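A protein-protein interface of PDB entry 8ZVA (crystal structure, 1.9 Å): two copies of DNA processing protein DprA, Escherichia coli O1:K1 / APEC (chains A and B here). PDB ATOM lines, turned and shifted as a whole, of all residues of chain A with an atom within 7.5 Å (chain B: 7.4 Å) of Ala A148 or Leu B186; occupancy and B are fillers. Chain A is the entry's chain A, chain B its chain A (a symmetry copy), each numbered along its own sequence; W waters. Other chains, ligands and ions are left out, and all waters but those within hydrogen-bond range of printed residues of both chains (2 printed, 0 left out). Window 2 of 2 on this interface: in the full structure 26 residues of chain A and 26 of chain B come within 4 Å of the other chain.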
ATOM      1  N   ASN A 145      25.986 -28.877 -21.947  1.00  0.00           N
ATOM      2  CA  ASN A 145      27.170 -28.284 -22.557  1.00  0.00           C
ATOM      3  C   ASN A 145      26.891 -26.817 -22.837  1.00  0.00           C
ATOM      4  O   ASN A 145      26.883 -26.371 -23.998  1.00  0.00           O
ATOM      5  CB  ASN A 145      27.548 -29.072 -23.805  1.00  0.00           C
ATOM      6  CG  ASN A 145      28.692 -29.978 -23.600  1.00  0.00           C
ATOM      7  OD1 ASN A 145      29.841 -29.600 -23.322  1.00  0.00           O
ATOM      8  ND2 ASN A 145      28.370 -31.249 -23.687  1.00  0.00           N
ATOM      9  N   PRO A 146      26.705 -26.027 -21.766  1.00  0.00           N
ATOM     10  CA  PRO A 146      26.280 -24.629 -21.903  1.00  0.00           C
ATOM     11  C   PRO A 146      27.415 -23.717 -22.345  1.00  0.00           C
ATOM     12  O   PRO A 146      28.599 -24.045 -22.253  1.00  0.00           O
ATOM     13  CB  PRO A 146      25.800 -24.264 -20.485  1.00  0.00           C
ATOM     14  CG  PRO A 146      26.623 -25.093 -19.577  1.00  0.00           C
ATOM     15  CD  PRO A 146      26.884 -26.410 -20.345  1.00  0.00           C
ATOM     16  N   THR A 147      27.016 -22.576 -22.895  1.00  0.00           N
ATOM     17  CA  THR A 147      27.940 -21.486 -23.145  1.00  0.00           C
ATOM     18  C   THR A 147      28.232 -20.766 -21.833  1.00  0.00           C
ATOM     19  O   THR A 147      27.617 -21.034 -20.796  1.00  0.00           O
ATOM     20  CB  THR A 147      27.361 -20.508 -24.169  1.00  0.00           C
ATOM     21  OG1 THR A 147      26.180 -19.901 -23.632  1.00  0.00           O
ATOM     22  CG2 THR A 147      27.012 -21.235 -25.461  1.00  0.00           C
ATOM     23  N   ALA A 148      29.183 -19.834 -21.886  1.00  0.00           N
ATOM     24  CA  ALA A 148      29.484 -19.032 -20.707  1.00  0.00           C
ATOM     25  C   ALA A 148      28.254 -18.267 -20.240  1.00  0.00           C
ATOM     26  O   ALA A 148      28.007 -18.149 -19.034  1.00  0.00           O
ATOM     27  CB  ALA A 148      30.632 -18.072 -21.010  1.00  0.00           C
ATOM     28  N   LEU A 149      27.465 -17.744 -21.181  1.00  0.00           N
ATOM     29  CA  LEU A 149      26.302 -16.944 -20.809  1.00  0.00           C
ATOM     30  C   LEU A 149      25.211 -17.807 -20.193  1.00  0.00           C
ATOM     31  O   LEU A 149      24.511 -17.366 -19.274  1.00  0.00           O
ATOM     32  CB  LEU A 149      25.770 -16.198 -22.031  1.00  0.00           C
ATOM     33  CG  LEU A 149      24.432 -15.479 -21.857  1.00  0.00           C
ATOM     34  CD1 LEU A 149      24.544 -14.376 -20.823  1.00  0.00           C
ATOM     35  CD2 LEU A 149      23.954 -14.922 -23.193  1.00  0.00           C
ATOM     36  N   GLY A 150      25.034 -19.029 -20.693  1.00  0.00           N
ATOM     37  CA  GLY A 150      24.080 -19.927 -20.068  1.00  0.00           C
ATOM     38  C   GLY A 150      24.413 -20.183 -18.610  1.00  0.00           C
ATOM     39  O   GLY A 150      23.527 -20.197 -17.752  1.00  0.00           O
ATOM     40  N   ILE A 151      25.699 -20.367 -18.310  1.00  0.00           N
ATOM     41  CA  ILE A 151      26.112 -20.601 -16.932  1.00  0.00           C
ATOM     42  C   ILE A 151      25.773 -19.398 -16.063  1.00  0.00           C
ATOM     43  O   ILE A 151      25.334 -19.547 -14.917  1.00  0.00           O
ATOM     44  CB  ILE A 151      27.614 -20.938 -16.873  1.00  0.00           C
ATOM     45  CG1 ILE A 151      27.875 -22.267 -17.583  1.00  0.00           C
ATOM     46  CG2 ILE A 151      28.091 -20.997 -15.429  1.00  0.00           C
ATOM     47  CD1 ILE A 151      29.337 -22.567 -17.818  1.00  0.00           C
ATOM     48  N   TYR A 152      25.976 -18.185 -16.583  1.00  0.00           N
ATOM     49  CA  TYR A 152      25.652 -17.012 -15.782  1.00  0.00           C
ATOM     50  C   TYR A 152      24.149 -16.890 -15.579  1.00  0.00           C
ATOM     51  O   TYR A 152      23.679 -16.672 -14.457  1.00  0.00           O
ATOM     52  CB  TYR A 152      26.173 -15.732 -16.424  1.00  0.00           C
ATOM     53  CG  TYR A 152      25.594 -14.512 -15.733  1.00  0.00           C
ATOM     54  CD1 TYR A 152      26.060 -14.117 -14.486  1.00  0.00           C
ATOM     55  CD2 TYR A 152      24.558 -13.783 -16.305  1.00  0.00           C
ATOM     56  CE1 TYR A 152      25.532 -13.017 -13.839  1.00  0.00           C
ATOM     57  CE2 TYR A 152      24.022 -12.679 -15.663  1.00  0.00           C
ATOM     58  CZ  TYR A 152      24.513 -12.303 -14.430  1.00  0.00           C
ATOM     59  OH  TYR A 152      23.988 -11.207 -13.784  1.00  0.00           O
ATOM     60  N   LEU A 153      23.381 -16.993 -16.668  1.00  0.00           N
ATOM     61  CA  LEU A 153      21.934 -16.842 -16.572  1.00  0.00           C
ATOM     62  C   LEU A 153      21.353 -17.797 -15.540  1.00  0.00           C
ATOM     63  O   LEU A 153      20.435 -17.436 -14.795  1.00  0.00           O
ATOM     64  CB  LEU A 153      21.292 -17.078 -17.939  1.00  0.00           C
ATOM     65  CG  LEU A 153      21.485 -15.989 -18.995  1.00  0.00           C
ATOM     66  CD1 LEU A 153      20.861 -16.434 -20.316  1.00  0.00           C
ATOM     67  CD2 LEU A 153      20.893 -14.668 -18.543  1.00  0.00           C
ATOM     68  N   THR A 154      21.880 -19.021 -15.477  1.00  0.00           N
ATOM     69  CA  THR A 154      21.435 -19.971 -14.464  1.00  0.00           C
ATOM     70  C   THR A 154      21.555 -19.369 -13.069  1.00  0.00           C
ATOM     71  O   THR A 154      20.596 -19.379 -12.288  1.00  0.00           O
ATOM     72  CB  THR A 154      22.252 -21.261 -14.559  1.00  0.00           C
ATOM     73  OG1 THR A 154      22.143 -21.805 -15.881  1.00  0.00           O
ATOM     74  CG2 THR A 154      21.759 -22.284 -13.548  1.00  0.00           C
ATOM     75  N   GLN A 155      22.734 -18.838 -12.740  1.00  0.00           N
ATOM     76  CA  GLN A 155      22.933 -18.238 -11.426  1.00  0.00           C
ATOM     77  C   GLN A 155      22.046 -17.014 -11.242  1.00  0.00           C
ATOM     78  O   GLN A 155      21.423 -16.842 -10.188  1.00  0.00           O
ATOM     79  CB  GLN A 155      24.403 -17.863 -11.238  1.00  0.00           C
ATOM     80  CG  GLN A 155      25.377 -19.003 -11.482  1.00  0.00           C
ATOM     81  CD  GLN A 155      26.810 -18.523 -11.617  1.00  0.00           C
ATOM     82  OE1 GLN A 155      27.424 -18.079 -10.646  1.00  0.00           O
ATOM     83  NE2 GLN A 155      27.351 -18.609 -12.828  1.00  0.00           N
ATOM     84  N   GLU A 254      19.236 -22.673 -20.987  1.00  0.00           N
ATOM     85  CA  GLU A 254      19.856 -22.799 -22.304  1.00  0.00           C
ATOM     86  C   GLU A 254      19.583 -24.202 -22.826  1.00  0.00           C
ATOM     87  O   GLU A 254      19.937 -25.186 -22.168  1.00  0.00           O
ATOM     88  CB  GLU A 254      21.361 -22.530 -22.230  1.00  0.00           C
ATOM     89  CG  GLU A 254      22.054 -22.495 -23.580  1.00  0.00           C
ATOM     90  CD  GLU A 254      23.469 -21.957 -23.483  1.00  0.00           C
ATOM     91  OE1 GLU A 254      24.289 -22.572 -22.770  1.00  0.00           O
ATOM     92  OE2 GLU A 254      23.760 -20.920 -24.113  1.00  0.00           O
ATOM     93  N   LEU A 280      18.732 -12.298 -21.690  1.00  0.00           N
ATOM     94  CA  LEU A 280      19.603 -11.212 -21.265  1.00  0.00           C
ATOM     95  C   LEU A 280      19.156  -9.903 -21.902  1.00  0.00           C
ATOM     96  O   LEU A 280      18.714  -9.872 -23.054  1.00  0.00           O
ATOM     97  CB  LEU A 280      21.053 -11.515 -21.644  1.00  0.00           C
ATOM     98  CG  LEU A 280      22.109 -10.603 -21.015  1.00  0.00           C
ATOM     99  CD1 LEU A 280      22.345 -10.976 -19.559  1.00  0.00           C
ATOM    100  CD2 LEU A 280      23.410 -10.666 -21.804  1.00  0.00           C
ATOM    101  N   GLN B 155      29.940 -10.297 -11.586  1.00  0.00           N
ATOM    102  CA  GLN B 155      29.182 -10.435 -12.823  1.00  0.00           C
ATOM    103  C   GLN B 155      27.807  -9.793 -12.699  1.00  0.00           C
ATOM    104  O   GLN B 155      27.361  -9.083 -13.608  1.00  0.00           O
ATOM    105  CB  GLN B 155      29.047 -11.913 -13.193  1.00  0.00           C
ATOM    106  CG  GLN B 155      30.365 -12.665 -13.263  1.00  0.00           C
ATOM    107  CD  GLN B 155      30.174 -14.168 -13.296  1.00  0.00           C
ATOM    108  OE1 GLN B 155      29.696 -14.724 -14.286  1.00  0.00           O
ATOM    109  NE2 GLN B 155      30.548 -14.838 -12.211  1.00  0.00           N
ATOM    110  N   ILE B 162      24.244  -3.171 -18.659  1.00  0.00           N
ATOM    111  CA  ILE B 162      24.008  -3.536 -20.048  1.00  0.00           C
ATOM    112  C   ILE B 162      23.132  -2.479 -20.705  1.00  0.00           C
ATOM    113  O   ILE B 162      22.133  -2.022 -20.135  1.00  0.00           O
ATOM    114  CB  ILE B 162      23.363  -4.929 -20.134  1.00  0.00           C
ATOM    115  CG1 ILE B 162      24.360  -5.995 -19.670  1.00  0.00           C
ATOM    116  CG2 ILE B 162      22.898  -5.214 -21.554  1.00  0.00           C
ATOM    117  CD1 ILE B 162      23.746  -7.366 -19.460  1.00  0.00           C
ATOM    118  N   ALA B 180      35.783  -9.156 -13.523  1.00  0.00           N
ATOM    119  CA  ALA B 180      35.132  -7.950 -14.025  1.00  0.00           C
ATOM    120  C   ALA B 180      35.311  -7.826 -15.531  1.00  0.00           C
ATOM    121  O   ALA B 180      34.352  -7.551 -16.262  1.00  0.00           O
ATOM    122  CB  ALA B 180      35.693  -6.719 -13.313  1.00  0.00           C
ATOM    123  N   HIS B 181      36.539  -8.025 -16.016  1.00  0.00           N
ATOM    124  CA  HIS B 181      36.785  -7.967 -17.453  1.00  0.00           C
ATOM    125  C   HIS B 181      36.053  -9.089 -18.177  1.00  0.00           C
ATOM    126  O   HIS B 181      35.416  -8.861 -19.213  1.00  0.00           O
ATOM    127  CB  HIS B 181      38.286  -8.043 -17.727  1.00  0.00           C
ATOM    128  CG  HIS B 181      39.051  -6.853 -17.242  1.00  0.00           C
ATOM    129  ND1 HIS B 181      38.663  -5.558 -17.510  1.00  0.00           N
ATOM    130  CD2 HIS B 181      40.185  -6.762 -16.507  1.00  0.00           C
ATOM    131  CE1 HIS B 181      39.526  -4.720 -16.963  1.00  0.00           C
ATOM    132  NE2 HIS B 181      40.458  -5.424 -16.347  1.00  0.00           N
ATOM    133  N   GLU B 182      36.139 -10.312 -17.647  1.00  0.00           N
ATOM    134  CA  GLU B 182      35.436 -11.439 -18.254  1.00  0.00           C
ATOM    135  C   GLU B 182      33.938 -11.171 -18.334  1.00  0.00           C
ATOM    136  O   GLU B 182      33.291 -11.514 -19.330  1.00  0.00           O
ATOM    137  CB  GLU B 182      35.719 -12.711 -17.454  1.00  0.00           C
ATOM    138  CG  GLU B 182      35.064 -13.965 -18.007  1.00  0.00           C
ATOM    139  CD  GLU B 182      34.420 -14.804 -16.922  1.00  0.00           C
ATOM    140  OE1 GLU B 182      33.655 -14.234 -16.115  1.00  0.00           O
ATOM    141  OE2 GLU B 182      34.684 -16.026 -16.866  1.00  0.00           O
ATOM    142  N   ALA B 183      33.370 -10.552 -17.298  1.00  0.00           N
ATOM    143  CA  ALA B 183      31.942 -10.248 -17.311  1.00  0.00           C
ATOM    144  C   ALA B 183      31.620  -9.182 -18.350  1.00  0.00           C
ATOM    145  O   ALA B 183      30.663  -9.322 -19.120  1.00  0.00           O
ATOM    146  CB  ALA B 183      31.487  -9.801 -15.920  1.00  0.00           C
ATOM    147  N   SER B 184      32.407  -8.102 -18.384  1.00  0.00           N
ATOM    148  CA  SER B 184      32.176  -7.049 -19.366  1.00  0.00           C
ATOM    149  C   SER B 184      32.205  -7.610 -20.782  1.00  0.00           C
ATOM    150  O   SER B 184      31.335  -7.301 -21.605  1.00  0.00           O
ATOM    151  CB  SER B 184      33.223  -5.947 -19.209  1.00  0.00           C
ATOM    152  OG  SER B 184      33.164  -5.372 -17.918  1.00  0.00           O
ATOM    153  N   LEU B 185      33.209  -8.435 -21.085  1.00  0.00           N
ATOM    154  CA  LEU B 185      33.282  -9.063 -22.399  1.00  0.00           C
ATOM    155  C   LEU B 185      32.036  -9.896 -22.671  1.00  0.00           C
ATOM    156  O   LEU B 185      31.450  -9.825 -23.758  1.00  0.00           O
ATOM    157  CB  LEU B 185      34.537  -9.931 -22.491  1.00  0.00           C
ATOM    158  CG  LEU B 185      35.884  -9.207 -22.476  1.00  0.00           C
ATOM    159  CD1 LEU B 185      37.025 -10.207 -22.350  1.00  0.00           C
ATOM    160  CD2 LEU B 185      36.044  -8.363 -23.728  1.00  0.00           C
ATOM    161  N   LEU B 186      31.610 -10.690 -21.684  1.00  0.00           N
ATOM    162  CA  LEU B 186      30.456 -11.562 -21.876  1.00  0.00           C
ATOM    163  C   LEU B 186      29.204 -10.761 -22.213  1.00  0.00           C
ATOM    164  O   LEU B 186      28.427 -11.153 -23.091  1.00  0.00           O
ATOM    165  CB  LEU B 186      30.229 -12.403 -20.620  1.00  0.00           C
ATOM    166  CG  LEU B 186      29.044 -13.372 -20.618  1.00  0.00           C
ATOM    167  CD1 LEU B 186      29.213 -14.438 -21.683  1.00  0.00           C
ATOM    168  CD2 LEU B 186      28.887 -14.002 -19.240  1.00  0.00           C
ATOM    169  N   PHE B 187      28.991  -9.641 -21.527  1.00  0.00           N
ATOM    170  CA  PHE B 187      27.815  -8.808 -21.745  1.00  0.00           C
ATOM    171  C   PHE B 187      28.047  -7.720 -22.786  1.00  0.00           C
ATOM    172  O   PHE B 187      27.179  -6.862 -22.973  1.00  0.00           O
ATOM    173  CB  PHE B 187      27.370  -8.175 -20.425  1.00  0.00           C
ATOM    174  CG  PHE B 187      27.187  -9.164 -19.307  1.00  0.00           C
ATOM    175  CD1 PHE B 187      26.590 -10.392 -19.539  1.00  0.00           C
ATOM    176  CD2 PHE B 187      27.610  -8.863 -18.024  1.00  0.00           C
ATOM    177  CE1 PHE B 187      26.422 -11.303 -18.513  1.00  0.00           C
ATOM    178  CE2 PHE B 187      27.444  -9.770 -16.993  1.00  0.00           C
ATOM    179  CZ  PHE B 187      26.850 -10.990 -17.239  1.00  0.00           C
ATOM    180  N   LYS B 188      29.198  -7.733 -23.460  1.00  0.00           N
ATOM    181  CA  LYS B 188      29.500  -6.788 -24.534  1.00  0.00           C
ATOM    182  C   LYS B 188      29.546  -5.347 -24.037  1.00  0.00           C
ATOM    183  O   LYS B 188      29.170  -4.418 -24.757  1.00  0.00           O
ATOM    184  CB  LYS B 188      28.498  -6.913 -25.682  1.00  0.00           C
ATOM    185  CG  LYS B 188      28.400  -8.304 -26.279  1.00  0.00           C
ATOM    186  CD  LYS B 188      27.522  -8.307 -27.521  1.00  0.00           C
ATOM    187  CE  LYS B 188      27.493  -9.679 -28.176  1.00  0.00           C
ATOM    188  NZ  LYS B 188      26.878  -9.639 -29.533  1.00  0.00           N
ATOM    189  N   ILE B 189      30.003  -5.143 -22.806  1.00  0.00           N
ATOM    190  CA  ILE B 189      30.283  -3.815 -22.282  1.00  0.00           C
ATOM    191  C   ILE B 189      31.768  -3.537 -22.511  1.00  0.00           C
ATOM    192  O   ILE B 189      32.603  -4.343 -22.071  1.00  0.00           O
ATOM    193  CB  ILE B 189      29.931  -3.703 -20.795  1.00  0.00           C
ATOM    194  CG1 ILE B 189      28.439  -3.968 -20.576  1.00  0.00           C
ATOM    195  CG2 ILE B 189      30.308  -2.332 -20.256  1.00  0.00           C
ATOM    196  CD1 ILE B 189      28.063  -4.192 -19.122  1.00  0.00           C
ATOM    197  N   ASN B 217      36.879  -6.057 -28.730  1.00  0.00           N
ATOM    198  CA  ASN B 217      35.520  -5.682 -28.367  1.00  0.00           C
ATOM    199  C   ASN B 217      35.387  -4.192 -28.080  1.00  0.00           C
ATOM    200  O   ASN B 217      34.481  -3.783 -27.345  1.00  0.00           O
ATOM    201  CB  ASN B 217      35.055  -6.500 -27.162  1.00  0.00           C
ATOM    202  CG  ASN B 217      34.640  -7.908 -27.542  1.00  0.00           C
ATOM    203  OD1 ASN B 217      33.452  -8.206 -27.656  1.00  0.00           O
ATOM    204  ND2 ASN B 217      35.620  -8.781 -27.745  1.00  0.00           N
HETATM  205  O   HOH W   1      30.105 -17.402 -10.804  1.00  0.00           O
HETATM  206  O   HOH W   2      29.538 -17.483 -14.472  1.00  0.00           O
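1 position is printed for both chains. Of the 6 pairs that touch across the chains among the printed residues, none has its exchanged pair printed and touching as well.
Of the 13 printed residues of chain B, 4 touch a printed residue of chain A. Hydrophobic or aromatic side chains of chain B within 4 Å of the printed part of chain A: Ile B162, Leu B186 and Phe B187. Along chain B the printed residues that touch a printed residue of chain A span positions 155 to 187.
Water W1 lies within hydrogen-bond range of the side-chain amide oxygen of Gln A155 (2.8 Å) and the side-chain amide nitrogen of Gln B155 (3.0 Å). Water W2 lies within hydrogen-bond range of the side-chain amide oxygen of Gln B155 (2.8 Å) and the side-chain amide nitrogen of Gln A155 (3.0 Å).
Ala A148 touches Leu B186 (CB to CD1, 3.96 Å). CD1 of Leu B186 touches N of Leu A149 (3.8 Å). CD1 of Tyr A152 touches OE1 of Gln B155, at 3.7 Å. Phe B187 touches Tyr A152. Leu A280 touches Ile B162 (CD1 to CD1, 3.9 Å). Phe B187 touches Leu A280 (CD1 to CD2, 3.9 Å).
Of the printed residues of chain B, Leu A149 touches Leu B186 (3.8 Å). Printed residues of chain A within 4 Å of Gln B155: Tyr A152. Of the printed residues of chain A, Ile B162 touches Leu A280. Glu B182 touches none of the printed residues of chain A. Of chain A, only Ala A148 and Leu A149 come within 4 Å of Leu B186. Printed residues of chain A within 4 Å of Phe B187: Tyr A152 and Leu A280.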
